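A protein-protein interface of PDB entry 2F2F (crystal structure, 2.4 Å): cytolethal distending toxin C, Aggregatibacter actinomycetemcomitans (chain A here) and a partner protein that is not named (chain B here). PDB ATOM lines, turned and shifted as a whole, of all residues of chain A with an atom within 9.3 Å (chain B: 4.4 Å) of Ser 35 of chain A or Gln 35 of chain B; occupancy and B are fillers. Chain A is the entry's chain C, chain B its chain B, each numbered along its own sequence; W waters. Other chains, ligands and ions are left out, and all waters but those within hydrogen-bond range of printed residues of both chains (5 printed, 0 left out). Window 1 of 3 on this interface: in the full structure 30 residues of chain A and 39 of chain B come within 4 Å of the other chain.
OE1 of Gln 35 of chain B lies close to OG of Ser 35 of chain A (3.3 Å).
Of the printed residues of chain B, Val 32 of chain A touches Glu 66 (3.5 Å).
Of the printed residues of chain B, Leu 34 of chain A touches Ser 37.
Gln 35 of chain B touches one residue of chain A.
Gly 36 of chain B touches none of the printed residues of chain A.
Printed residues of chain A within 4 Å of Ser 37 of chain B: Leu 34.
Printed residues of chain A within 4 Å of Glu 66 of chain B: Val 32 (3.5 Å).
The nearest printed residue of chain B that does not touch Ser 35 of chain A is Ser 37 of chain B (4.5 Å).
The nearest printed residue of chain B that does not touch Val 32 of chain A is Asn 33 of chain B (6.3 Å).
Of the 11 printed residues of chain A, 3 touch a printed residue of chain B.
Hydrophobic or aromatic side chains of chain A within 4 Å of the printed part of chain B: Val 32 and Leu 34.
Printed residues of chain B that touch a printed residue of chain A: Gln 35, Ser 37 and Glu 66.
Among the printed residues, no Asp or Glu carboxylate lies within 4 Å of a Lys or Arg side-chain nitrogen of the other chain.
The backbone NH of Gln 35 of chain B lies within hydrogen-bond range of the side-chain amide oxygen of Asn 33 of chain B (3.0 Å).
OE2 of Glu 66 of chain B is in hydrogen-bond range of ND2 of Asn 33 of chain B (3.0 Å).
The backbone carbonyl oxygen (O) of Gln 35 of chain B is in hydrogen-bond range of the side-chain amino group (NZ) of Lys 44 of chain B, at 3.2 Å.
The side-chain amide oxygen of Gln 35 of chain B sits at hydrogen-bond distance from the backbone NH of Asp 273 of chain B (3.0 Å).
The backbone NH (N) of Gly 36 of chain B lies within hydrogen-bond range of the backbone carbonyl oxygen (O) of Glu 66 of chain B, 2.9 Å away.
Among the printed residues, pairs that only touch across the chains: Val 32 of chain A with Glu 66 of chain B and Leu 34 of chain A with Ser 37 of chain B.
Water W5 bridges O of Ser 35 of chain A (2.5 Å) and OG of Ser 37 of chain B (2.9 Å).
Water W4 lies within hydrogen-bond range of NZ of Lys 44 of chain B (2.6 Å) and O of Pro 36 of chain A (2.7 Å).
Water W2 lies within hydrogen-bond range of the backbone carbonyl oxygen of Glu 33 of chain A, the side-chain carboxylate of Glu 66 of chain B and the side-chain hydroxyl of Ser 35 of chain A.
Water W3 lies within hydrogen-bond range of the backbone carbonyl oxygen of Gly 36 of chain B (2.7 Å) and the backbone NH of Ser 35 of chain A (3.0 Å).
Water W1 lies within hydrogen-bond range of O of Gln 35 of chain B (2.8 Å), OG of Ser 37 of chain B (2.8 Å) and O of Ser 35 of chain A (3.4 Å).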
ATOM      1  N   ASP A  25     -10.274  27.101 -14.119  1.00  0.00           N
ATOM      2  CA  ASP A  25      -8.802  27.330 -14.309  1.00  0.00           C
ATOM      3  C   ASP A  25      -8.423  28.779 -13.903  1.00  0.00           C
ATOM      4  O   ASP A  25      -8.657  29.129 -12.753  1.00  0.00           O
ATOM      5  CB  ASP A  25      -8.437  26.999 -15.759  1.00  0.00           C
ATOM      6  CG  ASP A  25      -7.044  26.410 -15.883  1.00  0.00           C
ATOM      7  OD1 ASP A  25      -6.316  26.404 -14.864  1.00  0.00           O
ATOM      8  OD2 ASP A  25      -6.676  25.960 -16.994  1.00  0.00           O
ATOM      9  N   VAL A  32     -17.062  30.385  -9.164  1.00  0.00           N
ATOM     10  CA  VAL A  32     -17.663  29.393 -10.048  1.00  0.00           C
ATOM     11  C   VAL A  32     -16.679  28.240 -10.295  1.00  0.00           C
ATOM     12  O   VAL A  32     -15.741  28.344 -11.099  1.00  0.00           O
ATOM     13  CB  VAL A  32     -18.069  30.059 -11.399  1.00  0.00           C
ATOM     14  CG1 VAL A  32     -18.692  29.017 -12.342  1.00  0.00           C
ATOM     15  CG2 VAL A  32     -19.056  31.185 -11.142  1.00  0.00           C
ATOM     16  N   GLU A  33     -16.903  27.137  -9.589  1.00  0.00           N
ATOM     17  CA  GLU A  33     -16.057  25.951  -9.716  1.00  0.00           C
ATOM     18  C   GLU A  33     -16.120  25.296 -11.092  1.00  0.00           C
ATOM     19  O   GLU A  33     -17.181  25.224 -11.708  1.00  0.00           O
ATOM     20  CB  GLU A  33     -16.435  24.923  -8.652  1.00  0.00           C
ATOM     21  CG  GLU A  33     -15.389  23.824  -8.484  1.00  0.00           C
ATOM     22  CD  GLU A  33     -15.796  22.761  -7.470  1.00  0.00           C
ATOM     23  OE1 GLU A  33     -15.235  21.637  -7.528  1.00  0.00           O
ATOM     24  OE2 GLU A  33     -16.674  23.052  -6.622  1.00  0.00           O
ATOM     25  N   LEU A  34     -14.967  24.827 -11.562  1.00  0.00           N
ATOM     26  CA  LEU A  34     -14.864  24.176 -12.862  1.00  0.00           C
ATOM     27  C   LEU A  34     -15.675  22.885 -12.825  1.00  0.00           C
ATOM     28  O   LEU A  34     -15.730  22.215 -11.813  1.00  0.00           O
ATOM     29  CB  LEU A  34     -13.393  23.868 -13.184  1.00  0.00           C
ATOM     30  CG  LEU A  34     -12.974  23.230 -14.521  1.00  0.00           C
ATOM     31  CD1 LEU A  34     -13.007  24.214 -15.664  1.00  0.00           C
ATOM     32  CD2 LEU A  34     -11.566  22.697 -14.354  1.00  0.00           C
ATOM     33  N   SER A  35     -16.316  22.565 -13.936  1.00  0.00           N
ATOM     34  CA  SER A  35     -17.122  21.374 -14.039  1.00  0.00           C
ATOM     35  C   SER A  35     -16.402  20.296 -14.851  1.00  0.00           C
ATOM     36  O   SER A  35     -15.723  20.581 -15.834  1.00  0.00           O
ATOM     37  CB  SER A  35     -18.457  21.694 -14.699  1.00  0.00           C
ATOM     38  OG  SER A  35     -19.379  22.186 -13.745  1.00  0.00           O
ATOM     39  N   PRO A  36     -16.523  19.031 -14.417  1.00  0.00           N
ATOM     40  CA  PRO A  36     -15.899  17.893 -15.101  1.00  0.00           C
ATOM     41  C   PRO A  36     -16.651  17.562 -16.396  1.00  0.00           C
ATOM     42  O   PRO A  36     -17.766  18.019 -16.610  1.00  0.00           O
ATOM     43  CB  PRO A  36     -16.007  16.769 -14.087  1.00  0.00           C
ATOM     44  CG  PRO A  36     -17.234  17.117 -13.286  1.00  0.00           C
ATOM     45  CD  PRO A  36     -17.254  18.616 -13.207  1.00  0.00           C
ATOM     46  N   PRO A  37     -16.026  16.786 -17.286  1.00  0.00           N
ATOM     47  CA  PRO A  37     -16.725  16.453 -18.528  1.00  0.00           C
ATOM     48  C   PRO A  37     -18.001  15.669 -18.258  1.00  0.00           C
ATOM     49  O   PRO A  37     -18.143  15.041 -17.205  1.00  0.00           O
ATOM     50  CB  PRO A  37     -15.701  15.634 -19.313  1.00  0.00           C
ATOM     51  CG  PRO A  37     -14.358  15.964 -18.685  1.00  0.00           C
ATOM     52  CD  PRO A  37     -14.671  16.205 -17.240  1.00  0.00           C
ATOM     53  N   PRO A  38     -18.959  15.720 -19.192  1.00  0.00           N
ATOM     54  CA  PRO A  38     -20.221  14.997 -19.025  1.00  0.00           C
ATOM     55  C   PRO A  38     -20.080  13.477 -19.261  1.00  0.00           C
ATOM     56  O   PRO A  38     -19.298  13.024 -20.103  1.00  0.00           O
ATOM     57  CB  PRO A  38     -21.144  15.635 -20.057  1.00  0.00           C
ATOM     58  CG  PRO A  38     -20.253  16.228 -21.079  1.00  0.00           C
ATOM     59  CD  PRO A  38     -18.915  16.493 -20.442  1.00  0.00           C
ATOM     60  N   GLU A  67     -16.681   9.715 -21.189  1.00  0.00           N
ATOM     61  CA  GLU A  67     -16.650  11.129 -20.852  1.00  0.00           C
ATOM     62  C   GLU A  67     -16.594  11.832 -22.183  1.00  0.00           C
ATOM     63  O   GLU A  67     -15.765  11.489 -23.024  1.00  0.00           O
ATOM     64  CB  GLU A  67     -15.405  11.476 -20.054  1.00  0.00           C
ATOM     65  CG  GLU A  67     -15.617  11.417 -18.577  1.00  0.00           C
ATOM     66  CD  GLU A  67     -14.359  11.739 -17.802  1.00  0.00           C
ATOM     67  OE1 GLU A  67     -13.343  12.135 -18.420  1.00  0.00           O
ATOM     68  OE2 GLU A  67     -14.381  11.602 -16.558  1.00  0.00           O
ATOM     69  N   LEU A  68     -17.481  12.789 -22.402  1.00  0.00           N
ATOM     70  CA  LEU A  68     -17.454  13.507 -23.659  1.00  0.00           C
ATOM     71  C   LEU A  68     -16.516  14.701 -23.523  1.00  0.00           C
ATOM     72  O   LEU A  68     -16.732  15.576 -22.683  1.00  0.00           O
ATOM     73  CB  LEU A  68     -18.855  13.983 -24.039  1.00  0.00           C
ATOM     74  CG  LEU A  68     -18.941  14.717 -25.374  1.00  0.00           C
ATOM     75  CD1 LEU A  68     -18.537  13.804 -26.527  1.00  0.00           C
ATOM     76  CD2 LEU A  68     -20.351  15.199 -25.541  1.00  0.00           C
ATOM     77  N   ILE A  69     -15.458  14.720 -24.323  1.00  0.00           N
ATOM     78  CA  ILE A  69     -14.512  15.829 -24.289  1.00  0.00           C
ATOM     79  C   ILE A  69     -14.322  16.332 -25.712  1.00  0.00           C
ATOM     80  O   ILE A  69     -14.280  15.546 -26.660  1.00  0.00           O
ATOM     81  CB  ILE A  69     -13.122  15.409 -23.690  1.00  0.00           C
ATOM     82  CG1 ILE A  69     -12.416  14.423 -24.622  1.00  0.00           C
ATOM     83  CG2 ILE A  69     -13.302  14.784 -22.310  1.00  0.00           C
ATOM     84  CD1 ILE A  69     -11.066  13.947 -24.117  1.00  0.00           C
ATOM     85  N   ASN B  33     -27.721  26.774 -17.679  1.00  0.00           N
ATOM     86  CA  ASN B  33     -26.344  27.028 -17.302  1.00  0.00           C
ATOM     87  C   ASN B  33     -25.561  25.915 -17.971  1.00  0.00           C
ATOM     88  O   ASN B  33     -25.598  24.765 -17.545  1.00  0.00           O
ATOM     89  CB  ASN B  33     -26.159  26.964 -15.800  1.00  0.00           C
ATOM     90  CG  ASN B  33     -24.754  27.299 -15.398  1.00  0.00           C
ATOM     91  OD1 ASN B  33     -23.823  27.089 -16.158  1.00  0.00           O
ATOM     92  ND2 ASN B  33     -24.589  27.834 -14.205  1.00  0.00           N
ATOM     93  N   LEU B  34     -24.872  26.274 -19.045  1.00  0.00           N
ATOM     94  CA  LEU B  34     -24.113  25.339 -19.865  1.00  0.00           C
ATOM     95  C   LEU B  34     -22.888  24.740 -19.173  1.00  0.00           C
ATOM     96  O   LEU B  34     -22.418  23.676 -19.582  1.00  0.00           O
ATOM     97  CB  LEU B  34     -23.694  26.054 -21.155  1.00  0.00           C
ATOM     98  CG  LEU B  34     -23.061  25.291 -22.317  1.00  0.00           C
ATOM     99  CD1 LEU B  34     -23.484  25.956 -23.602  1.00  0.00           C
ATOM    100  CD2 LEU B  34     -21.555  25.309 -22.216  1.00  0.00           C
ATOM    101  N   GLN B  35     -22.397  25.416 -18.132  1.00  0.00           N
ATOM    102  CA  GLN B  35     -21.213  25.007 -17.378  1.00  0.00           C
ATOM    103  C   GLN B  35     -20.057  24.699 -18.316  1.00  0.00           C
ATOM    104  O   GLN B  35     -19.396  23.668 -18.194  1.00  0.00           O
ATOM    105  CB  GLN B  35     -21.512  23.819 -16.490  1.00  0.00           C
ATOM    106  CG  GLN B  35     -22.107  24.221 -15.175  1.00  0.00           C
ATOM    107  CD  GLN B  35     -22.354  23.050 -14.276  1.00  0.00           C
ATOM    108  OE1 GLN B  35     -22.482  21.922 -14.742  1.00  0.00           O
ATOM    109  NE2 GLN B  35     -22.425  23.300 -12.982  1.00  0.00           N
ATOM    110  N   GLY B  36     -19.827  25.605 -19.266  1.00  0.00           N
ATOM    111  CA  GLY B  36     -18.772  25.434 -20.238  1.00  0.00           C
ATOM    112  C   GLY B  36     -17.387  25.432 -19.636  1.00  0.00           C
ATOM    113  O   GLY B  36     -17.195  25.737 -18.460  1.00  0.00           O
ATOM    114  N   SER B  37     -16.412  25.043 -20.443  1.00  0.00           N
ATOM    115  CA  SER B  37     -15.035  25.028 -19.991  1.00  0.00           C
ATOM    116  C   SER B  37     -14.198  24.774 -21.224  1.00  0.00           C
ATOM    117  O   SER B  37     -14.726  24.525 -22.299  1.00  0.00           O
ATOM    118  CB  SER B  37     -14.811  23.930 -18.958  1.00  0.00           C
ATOM    119  OG  SER B  37     -14.547  22.708 -19.600  1.00  0.00           O
ATOM    120  N   LYS B  44     -21.529  20.976 -26.074  1.00  0.00           N
ATOM    121  CA  LYS B  44     -22.724  21.317 -25.312  1.00  0.00           C
ATOM    122  C   LYS B  44     -23.687  22.184 -26.134  1.00  0.00           C
ATOM    123  O   LYS B  44     -24.900  22.025 -26.047  1.00  0.00           O
ATOM    124  CB  LYS B  44     -22.335  22.054 -24.039  1.00  0.00           C
ATOM    125  CG  LYS B  44     -21.350  21.295 -23.194  1.00  0.00           C
ATOM    126  CD  LYS B  44     -21.525  21.631 -21.732  1.00  0.00           C
ATOM    127  CE  LYS B  44     -20.364  21.097 -20.901  1.00  0.00           C
ATOM    128  NZ  LYS B  44     -20.682  21.049 -19.434  1.00  0.00           N
ATOM    129  N   GLN B  65     -25.769  30.687 -19.350  1.00  0.00           N
ATOM    130  CA  GLN B  65     -24.759  31.083 -18.368  1.00  0.00           C
ATOM    131  C   GLN B  65     -23.540  30.170 -18.557  1.00  0.00           C
ATOM    132  O   GLN B  65     -23.653  29.042 -19.060  1.00  0.00           O
ATOM    133  CB  GLN B  65     -25.280  30.922 -16.936  1.00  0.00           C
ATOM    134  CG  GLN B  65     -26.426  31.813 -16.567  1.00  0.00           C
ATOM    135  CD  GLN B  65     -27.750  31.188 -16.941  1.00  0.00           C
ATOM    136  OE1 GLN B  65     -27.978  30.007 -16.670  1.00  0.00           O
ATOM    137  NE2 GLN B  65     -28.629  31.967 -17.573  1.00  0.00           N
ATOM    138  N   GLU B  66     -22.375  30.666 -18.158  1.00  0.00           N
ATOM    139  CA  GLU B  66     -21.138  29.919 -18.291  1.00  0.00           C
ATOM    140  C   GLU B  66     -21.078  29.387 -19.715  1.00  0.00           C
ATOM    141  O   GLU B  66     -20.769  28.218 -19.939  1.00  0.00           O
ATOM    142  CB  GLU B  66     -21.112  28.760 -17.293  1.00  0.00           C
ATOM    143  CG  GLU B  66     -21.181  29.179 -15.825  1.00  0.00           C
ATOM    144  CD  GLU B  66     -20.976  28.015 -14.875  1.00  0.00           C
ATOM    145  OE1 GLU B  66     -20.108  27.175 -15.160  1.00  0.00           O
ATOM    146  OE2 GLU B  66     -21.663  27.923 -13.837  1.00  0.00           O
ATOM    147  N   SER B 272     -24.718  19.229 -18.716  1.00  0.00           N
ATOM    148  CA  SER B 272     -24.287  20.043 -17.574  1.00  0.00           C
ATOM    149  C   SER B 272     -25.035  19.520 -16.355  1.00  0.00           C
ATOM    150  O   SER B 272     -25.869  18.631 -16.490  1.00  0.00           O
ATOM    151  CB  SER B 272     -24.611  21.530 -17.817  1.00  0.00           C
ATOM    152  OG  SER B 272     -25.766  21.915 -17.101  1.00  0.00           O
ATOM    153  N   ASP B 273     -24.739  20.056 -15.174  1.00  0.00           N
ATOM    154  CA  ASP B 273     -25.403  19.636 -13.933  1.00  0.00           C
ATOM    155  C   ASP B 273     -26.677  20.432 -13.715  1.00  0.00           C
ATOM    156  O   ASP B 273     -27.380  20.250 -12.722  1.00  0.00           O
ATOM    157  CB  ASP B 273     -24.513  19.886 -12.717  1.00  0.00           C
ATOM    158  CG  ASP B 273     -23.378  18.888 -12.597  1.00  0.00           C
ATOM    159  OD1 ASP B 273     -23.273  17.969 -13.429  1.00  0.00           O
ATOM    160  OD2 ASP B 273     -22.573  19.033 -11.653  1.00  0.00           O
ATOM    161  N   HIS B 274     -26.934  21.356 -14.630  1.00  0.00           N
ATOM    162  CA  HIS B 274     -28.112  22.201 -14.546  1.00  0.00           C
ATOM    163  C   HIS B 274     -29.095  21.760 -15.603  1.00  0.00           C
ATOM    164  O   HIS B 274     -28.705  21.455 -16.739  1.00  0.00           O
ATOM    165  CB  HIS B 274     -27.730  23.671 -14.790  1.00  0.00           C
ATOM    166  CG  HIS B 274     -27.175  24.358 -13.575  1.00  0.00           C
ATOM    167  ND1 HIS B 274     -27.977  24.930 -12.612  1.00  0.00           N
ATOM    168  CD2 HIS B 274     -25.901  24.539 -13.162  1.00  0.00           C
ATOM    169  CE1 HIS B 274     -27.221  25.421 -11.651  1.00  0.00           C
ATOM    170  NE2 HIS B 274     -25.957  25.200 -11.959  1.00  0.00           N
HETATM  171  O   HOH W   1     -17.096  22.175 -18.527  1.00  0.00           O
HETATM  172  O   HOH W   2     -18.569  25.010 -13.982  1.00  0.00           O
HETATM  173  O   HOH W   3     -16.907  24.725 -15.970  1.00  0.00           O
HETATM  174  O   HOH W   4     -18.596  19.732 -18.528  1.00  0.00           O
HETATM  175  O   HOH W   5     -14.121  20.558 -17.728  1.00  0.00           O
